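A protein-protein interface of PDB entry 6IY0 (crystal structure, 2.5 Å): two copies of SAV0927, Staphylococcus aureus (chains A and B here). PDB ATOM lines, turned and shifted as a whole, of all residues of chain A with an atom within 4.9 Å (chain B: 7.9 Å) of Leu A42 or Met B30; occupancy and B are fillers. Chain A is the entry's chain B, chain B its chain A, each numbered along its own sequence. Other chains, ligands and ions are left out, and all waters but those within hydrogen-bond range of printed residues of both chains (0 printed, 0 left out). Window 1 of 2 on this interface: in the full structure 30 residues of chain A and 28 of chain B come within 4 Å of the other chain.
Among the printed residues, pairs that only touch across the chains: Met A30 with Leu B42 (3.5 Å), Val A32 with Met B30 (3.9 Å), Thr A34 with Phe B17 (3.5 Å), Thr A34 with Met B30 (3.9 Å), His A37 with Met B46 (3.9 Å), Leu A42 with Met B30 (3.6 Å), Leu A42 with Leu B44 (3.6 Å), Leu A44 with Leu B44 (3.8 Å), Leu A44 with Phe B51 (3.8 Å), Phe A51 with Leu B44 (3.7 Å), Phe A51 with Asn B45 (3.4 Å), Phe A51 with Met B46 (3.7 Å), Phe A51 with Lys B50 (3.4 Å) and Phe A51 with Phe B51 (3.8 Å).
Hydrophobic or aromatic side chains of chain A within 4 Å of the printed part of chain B: Met A30, Val A32, His A37, Leu A42, Leu A44 and Phe A51. Along chain A the printed residues that touch a printed residue of chain B span positions 30 to 51. Of the 24 printed residues of chain B, 8 touch a printed residue of chain A. Hydrophobic or aromatic side chains of chain B within 4 Å of the printed part of chain A: Phe B17, Met B30, Leu B42, Leu B44, Met B46 and Phe B51.
O of Asp B28 lies within hydrogen-bond range of N of Met B46 (3.1 Å). N of Leu B44 is in hydrogen-bond range of O of Met B30, at 2.8 Å. The backbone NH (N) of Val B32 sits at hydrogen-bond distance from the backbone carbonyl oxygen (O) of Leu B42, at 3.0 Å. The backbone carbonyl oxygen (O) of Lys B50 lies within hydrogen-bond range of the backbone NH (N) of Asn B45. The backbone carbonyl oxygen of Met A30 lies within hydrogen-bond range of the backbone NH of Leu A44 (2.7 Å). The backbone carbonyl oxygen (O) of Leu A42 lies within hydrogen-bond range of the backbone NH (N) of Val A32 (2.9 Å).
Met A30 touches Leu B42, and with the chains exchanged Leu A42 touches Met B30. Val A32 touches Met B30, but with the chains exchanged Met A30 does not touch Val B32 (5.0 Å). Leu A42 touches Leu B44, but with the chains exchanged Leu A44 does not touch Leu B42 (4.02 Å). Phe B51 touches its own counterpart, Phe A51. Positions printed for both chains: 30, 31, 32, 41, 42, 43, 44, 51 and 52.
Of the printed residues of chain B, Leu A42 touches Met B30 (3.6 Å) and Leu B44 (3.6 Å). Met B30 touches three residues of chain A. Printed residues of chain B within 4 Å of Val A32: Met B30 (3.9 Å). Of the printed residues of chain A, Asn B45 touches Phe A51. Of the printed residues of chain A, Met B46 touches His A37 and Phe A51. His B33 touches none of the printed residues of chain A. Leu B83 touches none of the printed residues of chain A. The nearest residue of chain B that does not touch Leu A42 is Met B46 (4.5 Å). The nearest residue of chain A that does not touch Met B30 is His A37 (4.1 Å). The nearest printed residue of chain A that does not touch Lys B50 is Gly A52 (7.2 Å).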
ATOM      1  N   MET A  30     -23.662   7.304 -16.692  1.00  0.00           N
ATOM      2  CA  MET A  30     -23.146   7.944 -15.496  1.00  0.00           C
ATOM      3  C   MET A  30     -22.232   6.984 -14.759  1.00  0.00           C
ATOM      4  O   MET A  30     -22.546   5.804 -14.601  1.00  0.00           O
ATOM      5  CB  MET A  30     -24.275   8.405 -14.578  1.00  0.00           C
ATOM      6  CG  MET A  30     -25.001   9.643 -15.046  1.00  0.00           C
ATOM      7  SD  MET A  30     -26.441  10.072 -13.819  1.00  0.00           S
ATOM      8  CE  MET A  30     -25.379  10.146 -12.200  1.00  0.00           C
ATOM      9  N   LEU A  31     -21.090   7.494 -14.312  1.00  0.00           N
ATOM     10  CA  LEU A  31     -20.097   6.695 -13.612  1.00  0.00           C
ATOM     11  C   LEU A  31     -19.915   7.263 -12.213  1.00  0.00           C
ATOM     12  O   LEU A  31     -19.512   8.420 -12.057  1.00  0.00           O
ATOM     13  CB  LEU A  31     -18.772   6.675 -14.378  1.00  0.00           C
ATOM     14  CG  LEU A  31     -18.572   5.517 -15.356  1.00  0.00           C
ATOM     15  CD1 LEU A  31     -19.615   5.524 -16.465  1.00  0.00           C
ATOM     16  CD2 LEU A  31     -17.176   5.567 -15.945  1.00  0.00           C
ATOM     17  N   VAL A  32     -20.226   6.455 -11.204  1.00  0.00           N
ATOM     18  CA  VAL A  32     -20.109   6.848  -9.806  1.00  0.00           C
ATOM     19  C   VAL A  32     -18.994   6.023  -9.183  1.00  0.00           C
ATOM     20  O   VAL A  32     -19.070   4.788  -9.147  1.00  0.00           O
ATOM     21  CB  VAL A  32     -21.431   6.652  -9.048  1.00  0.00           C
ATOM     22  CG1 VAL A  32     -21.340   7.257  -7.654  1.00  0.00           C
ATOM     23  CG2 VAL A  32     -22.588   7.260  -9.827  1.00  0.00           C
ATOM     24  N   THR A  34     -16.896   5.019  -5.819  1.00  0.00           N
ATOM     25  CA  THR A  34     -17.346   4.904  -4.444  1.00  0.00           C
ATOM     26  C   THR A  34     -16.442   3.928  -3.709  1.00  0.00           C
ATOM     27  O   THR A  34     -16.137   2.847  -4.221  1.00  0.00           O
ATOM     28  CB  THR A  34     -18.806   4.440  -4.402  1.00  0.00           C
ATOM     29  OG1 THR A  34     -19.658   5.512  -4.823  1.00  0.00           O
ATOM     30  CG2 THR A  34     -19.200   4.036  -3.012  1.00  0.00           C
ATOM     31  N   HIS A  37     -17.677   0.103  -2.776  1.00  0.00           N
ATOM     32  CA  HIS A  37     -17.661  -1.020  -3.703  1.00  0.00           C
ATOM     33  C   HIS A  37     -16.250  -1.502  -4.024  1.00  0.00           C
ATOM     34  O   HIS A  37     -16.048  -2.147  -5.059  1.00  0.00           O
ATOM     35  CB  HIS A  37     -18.400  -0.651  -4.988  1.00  0.00           C
ATOM     36  CG  HIS A  37     -19.801  -0.176  -4.758  1.00  0.00           C
ATOM     37  ND1 HIS A  37     -20.749  -0.941  -4.114  1.00  0.00           N
ATOM     38  CD2 HIS A  37     -20.414   0.987  -5.084  1.00  0.00           C
ATOM     39  CE1 HIS A  37     -21.886  -0.271  -4.053  1.00  0.00           C
ATOM     40  NE2 HIS A  37     -21.710   0.901  -4.635  1.00  0.00           N
ATOM     41  N   LYS A  40     -14.674  -0.876  -7.521  1.00  0.00           N
ATOM     42  CA  LYS A  40     -15.530  -1.100  -8.677  1.00  0.00           C
ATOM     43  C   LYS A  40     -16.374   0.139  -8.956  1.00  0.00           C
ATOM     44  O   LYS A  40     -16.817   0.828  -8.034  1.00  0.00           O
ATOM     45  CB  LYS A  40     -16.423  -2.321  -8.452  1.00  0.00           C
ATOM     46  CG  LYS A  40     -15.651  -3.607  -8.168  1.00  0.00           C
ATOM     47  CD  LYS A  40     -16.582  -4.762  -7.810  1.00  0.00           C
ATOM     48  CE  LYS A  40     -16.799  -4.874  -6.309  1.00  0.00           C
ATOM     49  NZ  LYS A  40     -18.206  -5.212  -5.961  1.00  0.00           N
ATOM     50  N   THR A  41     -16.592   0.418 -10.239  1.00  0.00           N
ATOM     51  CA  THR A  41     -17.258   1.639 -10.675  1.00  0.00           C
ATOM     52  C   THR A  41     -18.724   1.360 -10.984  1.00  0.00           C
ATOM     53  O   THR A  41     -19.051   0.360 -11.632  1.00  0.00           O
ATOM     54  CB  THR A  41     -16.562   2.230 -11.904  1.00  0.00           C
ATOM     55  OG1 THR A  41     -15.254   2.688 -11.539  1.00  0.00           O
ATOM     56  CG2 THR A  41     -17.357   3.401 -12.469  1.00  0.00           C
ATOM     57  N   LEU A  42     -19.599   2.243 -10.508  1.00  0.00           N
ATOM     58  CA  LEU A  42     -21.019   2.174 -10.820  1.00  0.00           C
ATOM     59  C   LEU A  42     -21.280   2.776 -12.196  1.00  0.00           C
ATOM     60  O   LEU A  42     -20.886   3.913 -12.466  1.00  0.00           O
ATOM     61  CB  LEU A  42     -21.822   2.920  -9.757  1.00  0.00           C
ATOM     62  CG  LEU A  42     -23.143   2.307  -9.305  1.00  0.00           C
ATOM     63  CD1 LEU A  42     -22.905   0.962  -8.650  1.00  0.00           C
ATOM     64  CD2 LEU A  42     -23.837   3.254  -8.349  1.00  0.00           C
ATOM     65  N   VAL A  43     -21.947   2.019 -13.061  1.00  0.00           N
ATOM     66  CA  VAL A  43     -22.240   2.446 -14.426  1.00  0.00           C
ATOM     67  C   VAL A  43     -23.753   2.526 -14.577  1.00  0.00           C
ATOM     68  O   VAL A  43     -24.440   1.497 -14.563  1.00  0.00           O
ATOM     69  CB  VAL A  43     -21.632   1.501 -15.471  1.00  0.00           C
ATOM     70  CG1 VAL A  43     -21.992   1.960 -16.874  1.00  0.00           C
ATOM     71  CG2 VAL A  43     -20.121   1.429 -15.302  1.00  0.00           C
ATOM     72  N   LEU A  44     -24.272   3.741 -14.721  1.00  0.00           N
ATOM     73  CA  LEU A  44     -25.698   3.978 -14.901  1.00  0.00           C
ATOM     74  C   LEU A  44     -25.993   4.253 -16.370  1.00  0.00           C
ATOM     75  O   LEU A  44     -25.239   4.964 -17.039  1.00  0.00           O
ATOM     76  CB  LEU A  44     -26.170   5.162 -14.052  1.00  0.00           C
ATOM     77  CG  LEU A  44     -26.521   4.956 -12.577  1.00  0.00           C
ATOM     78  CD1 LEU A  44     -25.280   4.660 -11.754  1.00  0.00           C
ATOM     79  CD2 LEU A  44     -27.242   6.184 -12.031  1.00  0.00           C
ATOM     80  N   PHE A  51     -28.479  -0.077 -13.986  1.00  0.00           N
ATOM     81  CA  PHE A  51     -27.092   0.114 -13.598  1.00  0.00           C
ATOM     82  C   PHE A  51     -26.508  -1.212 -13.138  1.00  0.00           C
ATOM     83  O   PHE A  51     -27.205  -2.224 -13.032  1.00  0.00           O
ATOM     84  CB  PHE A  51     -26.952   1.172 -12.495  1.00  0.00           C
ATOM     85  CG  PHE A  51     -27.479   0.734 -11.153  1.00  0.00           C
ATOM     86  CD1 PHE A  51     -28.807   0.937 -10.818  1.00  0.00           C
ATOM     87  CD2 PHE A  51     -26.641   0.137 -10.220  1.00  0.00           C
ATOM     88  CE1 PHE A  51     -29.294   0.549  -9.585  1.00  0.00           C
ATOM     89  CE2 PHE A  51     -27.125  -0.260  -8.986  1.00  0.00           C
ATOM     90  CZ  PHE A  51     -28.454  -0.053  -8.669  1.00  0.00           C
ATOM     91  N   GLY A  52     -25.209  -1.188 -12.856  1.00  0.00           N
ATOM     92  CA  GLY A  52     -24.520  -2.358 -12.351  1.00  0.00           C
ATOM     93  C   GLY A  52     -23.185  -1.981 -11.754  1.00  0.00           C
ATOM     94  O   GLY A  52     -22.552  -1.007 -12.174  1.00  0.00           O
ATOM     95  N   ILE A  53     -22.760  -2.752 -10.759  1.00  0.00           N
ATOM     96  CA  ILE A  53     -21.444  -2.575 -10.153  1.00  0.00           C
ATOM     97  C   ILE A  53     -20.436  -3.323 -11.019  1.00  0.00           C
ATOM     98  O   ILE A  53     -20.433  -4.557 -11.061  1.00  0.00           O
ATOM     99  CB  ILE A  53     -21.417  -3.074  -8.706  1.00  0.00           C
ATOM    100  CG1 ILE A  53     -22.621  -2.527  -7.938  1.00  0.00           C
ATOM    101  CG2 ILE A  53     -20.117  -2.666  -8.033  1.00  0.00           C
ATOM    102  CD1 ILE A  53     -22.528  -2.712  -6.445  1.00  0.00           C
ATOM    103  N   GLN B  14     -22.750  14.080  -2.829  1.00  0.00           N
ATOM    104  CA  GLN B  14     -22.928  13.290  -1.617  1.00  0.00           C
ATOM    105  C   GLN B  14     -23.799  12.080  -1.931  1.00  0.00           C
ATOM    106  O   GLN B  14     -24.965  12.229  -2.313  1.00  0.00           O
ATOM    107  CB  GLN B  14     -23.558  14.131  -0.506  1.00  0.00           C
ATOM    108  CG  GLN B  14     -23.112  15.585  -0.483  1.00  0.00           C
ATOM    109  CD  GLN B  14     -24.015  16.492  -1.300  1.00  0.00           C
ATOM    110  OE1 GLN B  14     -24.655  16.055  -2.258  1.00  0.00           O
ATOM    111  NE2 GLN B  14     -24.073  17.764  -0.921  1.00  0.00           N
ATOM    112  N   VAL B  15     -23.236  10.894  -1.777  1.00  0.00           N
ATOM    113  CA  VAL B  15     -23.975   9.653  -1.963  1.00  0.00           C
ATOM    114  C   VAL B  15     -24.495   9.192  -0.609  1.00  0.00           C
ATOM    115  O   VAL B  15     -23.773   9.231   0.393  1.00  0.00           O
ATOM    116  CB  VAL B  15     -23.091   8.580  -2.623  1.00  0.00           C
ATOM    117  CG1 VAL B  15     -23.722   7.212  -2.469  1.00  0.00           C
ATOM    118  CG2 VAL B  15     -22.875   8.908  -4.091  1.00  0.00           C
ATOM    119  N   GLN B  16     -25.753   8.763  -0.573  1.00  0.00           N
ATOM    120  CA  GLN B  16     -26.394   8.313   0.659  1.00  0.00           C
ATOM    121  C   GLN B  16     -26.820   6.858   0.495  1.00  0.00           C
ATOM    122  O   GLN B  16     -27.718   6.555  -0.298  1.00  0.00           O
ATOM    123  CB  GLN B  16     -27.587   9.201   1.011  1.00  0.00           C
ATOM    124  CG  GLN B  16     -28.388   8.712   2.202  1.00  0.00           C
ATOM    125  CD  GLN B  16     -29.456   9.698   2.636  1.00  0.00           C
ATOM    126  OE1 GLN B  16     -30.317   9.380   3.459  1.00  0.00           O
ATOM    127  NE2 GLN B  16     -29.403  10.905   2.087  1.00  0.00           N
ATOM    128  N   PHE B  17     -26.175   5.965   1.242  1.00  0.00           N
ATOM    129  CA  PHE B  17     -26.565   4.562   1.290  1.00  0.00           C
ATOM    130  C   PHE B  17     -27.554   4.368   2.432  1.00  0.00           C
ATOM    131  O   PHE B  17     -27.248   4.692   3.585  1.00  0.00           O
ATOM    132  CB  PHE B  17     -25.346   3.662   1.487  1.00  0.00           C
ATOM    133  CG  PHE B  17     -24.290   3.829   0.437  1.00  0.00           C
ATOM    134  CD1 PHE B  17     -23.237   4.707   0.631  1.00  0.00           C
ATOM    135  CD2 PHE B  17     -24.346   3.108  -0.740  1.00  0.00           C
ATOM    136  CE1 PHE B  17     -22.261   4.858  -0.331  1.00  0.00           C
ATOM    137  CE2 PHE B  17     -23.372   3.256  -1.704  1.00  0.00           C
ATOM    138  CZ  PHE B  17     -22.332   4.134  -1.502  1.00  0.00           C
ATOM    139  N   VAL B  18     -28.733   3.838   2.119  1.00  0.00           N
ATOM    140  CA  VAL B  18     -29.775   3.654   3.118  1.00  0.00           C
ATOM    141  C   VAL B  18     -30.326   2.240   3.037  1.00  0.00           C
ATOM    142  O   VAL B  18     -30.372   1.624   1.967  1.00  0.00           O
ATOM    143  CB  VAL B  18     -30.916   4.684   2.963  1.00  0.00           C
ATOM    144  CG1 VAL B  18     -30.442   6.055   3.402  1.00  0.00           C
ATOM    145  CG2 VAL B  18     -31.410   4.720   1.529  1.00  0.00           C
ATOM    146  N   GLY B  19     -30.747   1.730   4.189  1.00  0.00           N
ATOM    147  CA  GLY B  19     -31.389   0.437   4.272  1.00  0.00           C
ATOM    148  C   GLY B  19     -32.460   0.430   5.340  1.00  0.00           C
ATOM    149  O   GLY B  19     -32.224   0.870   6.470  1.00  0.00           O
ATOM    150  N   TYR B  27     -35.224  -3.270   2.086  1.00  0.00           N
ATOM    151  CA  TYR B  27     -34.838  -2.412   0.977  1.00  0.00           C
ATOM    152  C   TYR B  27     -33.466  -1.813   1.241  1.00  0.00           C
ATOM    153  O   TYR B  27     -33.158  -1.412   2.368  1.00  0.00           O
ATOM    154  CB  TYR B  27     -35.859  -1.291   0.761  1.00  0.00           C
ATOM    155  CG  TYR B  27     -37.288  -1.772   0.706  1.00  0.00           C
ATOM    156  CD1 TYR B  27     -37.882  -2.109  -0.504  1.00  0.00           C
ATOM    157  CD2 TYR B  27     -38.045  -1.889   1.863  1.00  0.00           C
ATOM    158  CE1 TYR B  27     -39.191  -2.549  -0.557  1.00  0.00           C
ATOM    159  CE2 TYR B  27     -39.350  -2.327   1.820  1.00  0.00           C
ATOM    160  CZ  TYR B  27     -39.919  -2.656   0.609  1.00  0.00           C
ATOM    161  OH  TYR B  27     -41.222  -3.092   0.569  1.00  0.00           O
ATOM    162  N   ASP B  28     -32.648  -1.756   0.193  1.00  0.00           N
ATOM    163  CA  ASP B  28     -31.328  -1.133   0.246  1.00  0.00           C
ATOM    164  C   ASP B  28     -31.218  -0.186  -0.940  1.00  0.00           C
ATOM    165  O   ASP B  28     -31.175  -0.632  -2.092  1.00  0.00           O
ATOM    166  CB  ASP B  28     -30.213  -2.180   0.217  1.00  0.00           C
ATOM    167  CG  ASP B  28     -30.359  -3.222   1.308  1.00  0.00           C
ATOM    168  OD1 ASP B  28     -31.033  -4.246   1.070  1.00  0.00           O
ATOM    169  OD2 ASP B  28     -29.796  -3.017   2.405  1.00  0.00           O
ATOM    170  N   LEU B  29     -31.176   1.113  -0.662  1.00  0.00           N
ATOM    171  CA  LEU B  29     -31.200   2.132  -1.697  1.00  0.00           C
ATOM    172  C   LEU B  29     -29.902   2.927  -1.691  1.00  0.00           C
ATOM    173  O   LEU B  29     -29.160   2.951  -0.706  1.00  0.00           O
ATOM    174  CB  LEU B  29     -32.389   3.091  -1.518  1.00  0.00           C
ATOM    175  CG  LEU B  29     -33.790   2.648  -1.959  1.00  0.00           C
ATOM    176  CD1 LEU B  29     -33.821   2.341  -3.450  1.00  0.00           C
ATOM    177  CD2 LEU B  29     -34.308   1.465  -1.149  1.00  0.00           C
ATOM    178  N   MET B  30     -29.640   3.579  -2.818  1.00  0.00           N
ATOM    179  CA  MET B  30     -28.522   4.501  -2.952  1.00  0.00           C
ATOM    180  C   MET B  30     -29.059   5.829  -3.474  1.00  0.00           C
ATOM    181  O   MET B  30     -29.801   5.862  -4.457  1.00  0.00           O
ATOM    182  CB  MET B  30     -27.457   3.928  -3.888  1.00  0.00           C
ATOM    183  CG  MET B  30     -26.148   4.702  -3.919  1.00  0.00           C
ATOM    184  SD  MET B  30     -24.731   3.677  -4.790  1.00  0.00           S
ATOM    185  CE  MET B  30     -23.520   5.125  -5.270  1.00  0.00           C
ATOM    186  N   LEU B  31     -28.701   6.923  -2.807  1.00  0.00           N
ATOM    187  CA  LEU B  31     -29.202   8.248  -3.149  1.00  0.00           C
ATOM    188  C   LEU B  31     -28.042   9.118  -3.609  1.00  0.00           C
ATOM    189  O   LEU B  31     -27.094   9.344  -2.850  1.00  0.00           O
ATOM    190  CB  LEU B  31     -29.922   8.888  -1.960  1.00  0.00           C
ATOM    191  CG  LEU B  31     -31.166   8.139  -1.482  1.00  0.00           C
ATOM    192  CD1 LEU B  31     -31.751   8.792  -0.239  1.00  0.00           C
ATOM    193  CD2 LEU B  31     -32.200   8.071  -2.591  1.00  0.00           C
ATOM    194  N   VAL B  32     -28.119   9.599  -4.847  1.00  0.00           N
ATOM    195  CA  VAL B  32     -27.111  10.480  -5.425  1.00  0.00           C
ATOM    196  C   VAL B  32     -27.737  11.858  -5.596  1.00  0.00           C
ATOM    197  O   VAL B  32     -28.751  12.006  -6.289  1.00  0.00           O
ATOM    198  CB  VAL B  32     -26.583   9.941  -6.764  1.00  0.00           C
ATOM    199  CG1 VAL B  32     -25.458  10.824  -7.282  1.00  0.00           C
ATOM    200  CG2 VAL B  32     -26.110   8.503  -6.610  1.00  0.00           C
ATOM    201  N   HIS B  33     -27.134  12.861  -4.964  1.00  0.00           N
ATOM    202  CA  HIS B  33     -27.617  14.239  -5.002  1.00  0.00           C
ATOM    203  C   HIS B  33     -26.685  15.045  -5.901  1.00  0.00           C
ATOM    204  O   HIS B  33     -25.575  15.401  -5.498  1.00  0.00           O
ATOM    205  CB  HIS B  33     -27.682  14.831  -3.596  1.00  0.00           C
ATOM    206  CG  HIS B  33     -28.523  14.039  -2.644  1.00  0.00           C
ATOM    207  ND1 HIS B  33     -29.874  14.259  -2.484  1.00  0.00           N
ATOM    208  CD2 HIS B  33     -28.204  13.026  -1.803  1.00  0.00           C
ATOM    209  CE1 HIS B  33     -30.352  13.417  -1.585  1.00  0.00           C
ATOM    210  NE2 HIS B  33     -29.358  12.658  -1.156  1.00  0.00           N
ATOM    211  N   THR B  41     -33.652  13.868  -7.214  1.00  0.00           N
ATOM    212  CA  THR B  41     -32.732  12.951  -6.557  1.00  0.00           C
ATOM    213  C   THR B  41     -32.646  11.637  -7.323  1.00  0.00           C
ATOM    214  O   THR B  41     -33.641  11.164  -7.882  1.00  0.00           O
ATOM    215  CB  THR B  41     -33.168  12.676  -5.113  1.00  0.00           C
ATOM    216  OG1 THR B  41     -34.596  12.581  -5.054  1.00  0.00           O
ATOM    217  CG2 THR B  41     -32.706  13.797  -4.195  1.00  0.00           C
ATOM    218  N   LEU B  42     -31.451  11.054  -7.344  1.00  0.00           N
ATOM    219  CA  LEU B  42     -31.228   9.745  -7.946  1.00  0.00           C
ATOM    220  C   LEU B  42     -31.425   8.665  -6.890  1.00  0.00           C
ATOM    221  O   LEU B  42     -30.732   8.660  -5.867  1.00  0.00           O
ATOM    222  CB  LEU B  42     -29.822   9.654  -8.535  1.00  0.00           C
ATOM    223  CG  LEU B  42     -29.627  10.089  -9.982  1.00  0.00           C
ATOM    224  CD1 LEU B  42     -28.200  10.549 -10.163  1.00  0.00           C
ATOM    225  CD2 LEU B  42     -29.950   8.947 -10.931  1.00  0.00           C
ATOM    226  N   VAL B  43     -32.361   7.753  -7.135  1.00  0.00           N
ATOM    227  CA  VAL B  43     -32.642   6.646  -6.229  1.00  0.00           C
ATOM    228  C   VAL B  43     -32.289   5.352  -6.947  1.00  0.00           C
ATOM    229  O   VAL B  43     -32.898   5.022  -7.972  1.00  0.00           O
ATOM    230  CB  VAL B  43     -34.107   6.639  -5.766  1.00  0.00           C
ATOM    231  CG1 VAL B  43     -34.264   5.790  -4.512  1.00  0.00           C
ATOM    232  CG2 VAL B  43     -34.585   8.061  -5.516  1.00  0.00           C
ATOM    233  N   LEU B  44     -31.314   4.623  -6.410  1.00  0.00           N
ATOM    234  CA  LEU B  44     -30.830   3.382  -7.001  1.00  0.00           C
ATOM    235  C   LEU B  44     -31.225   2.213  -6.109  1.00  0.00           C
ATOM    236  O   LEU B  44     -30.837   2.166  -4.937  1.00  0.00           O
ATOM    237  CB  LEU B  44     -29.313   3.416  -7.191  1.00  0.00           C
ATOM    238  CG  LEU B  44     -28.748   4.194  -8.381  1.00  0.00           C
ATOM    239  CD1 LEU B  44     -28.766   5.693  -8.122  1.00  0.00           C
ATOM    240  CD2 LEU B  44     -27.345   3.721  -8.701  1.00  0.00           C
ATOM    241  N   ASN B  45     -31.984   1.272  -6.665  1.00  0.00           N
ATOM    242  CA  ASN B  45     -32.358   0.054  -5.951  1.00  0.00           C
ATOM    243  C   ASN B  45     -31.256  -0.983  -6.146  1.00  0.00           C
ATOM    244  O   ASN B  45     -31.113  -1.546  -7.236  1.00  0.00           O
ATOM    245  CB  ASN B  45     -33.705  -0.460  -6.454  1.00  0.00           C
ATOM    246  CG  ASN B  45     -34.321  -1.500  -5.535  1.00  0.00           C
ATOM    247  OD1 ASN B  45     -33.616  -2.298  -4.920  1.00  0.00           O
ATOM    248  ND2 ASN B  45     -35.646  -1.489  -5.436  1.00  0.00           N
ATOM    249  N   MET B  46     -30.478  -1.242  -5.098  1.00  0.00           N
ATOM    250  CA  MET B  46     -29.329  -2.140  -5.208  1.00  0.00           C
ATOM    251  C   MET B  46     -29.712  -3.614  -5.350  1.00  0.00           C
ATOM    252  O   MET B  46     -28.871  -4.442  -5.696  1.00  0.00           O
ATOM    253  CB  MET B  46     -28.403  -1.981  -3.998  1.00  0.00           C
ATOM    254  CG  MET B  46     -28.048  -0.547  -3.640  1.00  0.00           C
ATOM    255  SD  MET B  46     -27.337   0.445  -5.153  1.00  0.00           S
ATOM    256  CE  MET B  46     -25.558  -0.345  -5.278  1.00  0.00           C
ATOM    257  N   LYS B  50     -32.093  -1.208 -10.750  1.00  0.00           N
ATOM    258  CA  LYS B  50     -32.751  -0.184 -11.543  1.00  0.00           C
ATOM    259  C   LYS B  50     -32.724   1.127 -10.768  1.00  0.00           C
ATOM    260  O   LYS B  50     -32.690   1.133  -9.533  1.00  0.00           O
ATOM    261  CB  LYS B  50     -34.198  -0.575 -11.883  1.00  0.00           C
ATOM    262  CG  LYS B  50     -34.364  -1.121 -13.295  1.00  0.00           C
ATOM    263  CD  LYS B  50     -35.816  -1.407 -13.659  1.00  0.00           C
ATOM    264  CE  LYS B  50     -36.724  -0.216 -13.400  1.00  0.00           C
ATOM    265  NZ  LYS B  50     -36.192   1.062 -13.956  1.00  0.00           N
ATOM    266  N   PHE B  51     -32.724   2.239 -11.498  1.00  0.00           N
ATOM    267  CA  PHE B  51     -32.678   3.554 -10.875  1.00  0.00           C
ATOM    268  C   PHE B  51     -33.672   4.478 -11.560  1.00  0.00           C
ATOM    269  O   PHE B  51     -34.182   4.192 -12.646  1.00  0.00           O
ATOM    270  CB  PHE B  51     -31.267   4.156 -10.922  1.00  0.00           C
ATOM    271  CG  PHE B  51     -30.815   4.553 -12.299  1.00  0.00           C
ATOM    272  CD1 PHE B  51     -30.184   3.642 -13.126  1.00  0.00           C
ATOM    273  CD2 PHE B  51     -31.015   5.845 -12.761  1.00  0.00           C
ATOM    274  CE1 PHE B  51     -29.763   4.011 -14.389  1.00  0.00           C
ATOM    275  CE2 PHE B  51     -30.600   6.216 -14.022  1.00  0.00           C
ATOM    276  CZ  PHE B  51     -29.974   5.299 -14.837  1.00  0.00           C
ATOM    277  N   GLY B  52     -33.935   5.607 -10.907  1.00  0.00           N
ATOM    278  CA  GLY B  52     -34.826   6.606 -11.456  1.00  0.00           C
ATOM    279  C   GLY B  52     -34.559   7.959 -10.830  1.00  0.00           C
ATOM    280  O   GLY B  52     -34.055   8.049  -9.710  1.00  0.00           O
ATOM    281  N   LEU B  69     -38.494   1.370 -10.177  1.00  0.00           N
ATOM    282  CA  LEU B  69     -37.540   0.624  -9.374  1.00  0.00           C
ATOM    283  C   LEU B  69     -37.702  -0.883  -9.505  1.00  0.00           C
ATOM    284  O   LEU B  69     -36.958  -1.629  -8.860  1.00  0.00           O
ATOM    285  CB  LEU B  69     -37.649   1.037  -7.900  1.00  0.00           C
ATOM    286  CG  LEU B  69     -37.151   2.449  -7.581  1.00  0.00           C
ATOM    287  CD1 LEU B  69     -37.019   2.656  -6.079  1.00  0.00           C
ATOM    288  CD2 LEU B  69     -35.831   2.730  -8.289  1.00  0.00           C
ATOM    289  N   LEU B  83     -39.161   7.673   0.761  1.00  0.00           N
ATOM    290  CA  LEU B  83     -38.577   8.691  -0.105  1.00  0.00           C
ATOM    291  C   LEU B  83     -39.161  10.074   0.159  1.00  0.00           C
ATOM    292  O   LEU B  83     -38.417  11.061   0.201  1.00  0.00           O
ATOM    293  CB  LEU B  83     -38.767   8.301  -1.572  1.00  0.00           C
ATOM    294  CG  LEU B  83     -37.759   7.291  -2.125  1.00  0.00           C
ATOM    295  CD1 LEU B  83     -37.958   7.092  -3.621  1.00  0.00           C
ATOM    296  CD2 LEU B  83     -36.331   7.719  -1.820  1.00  0.00           C
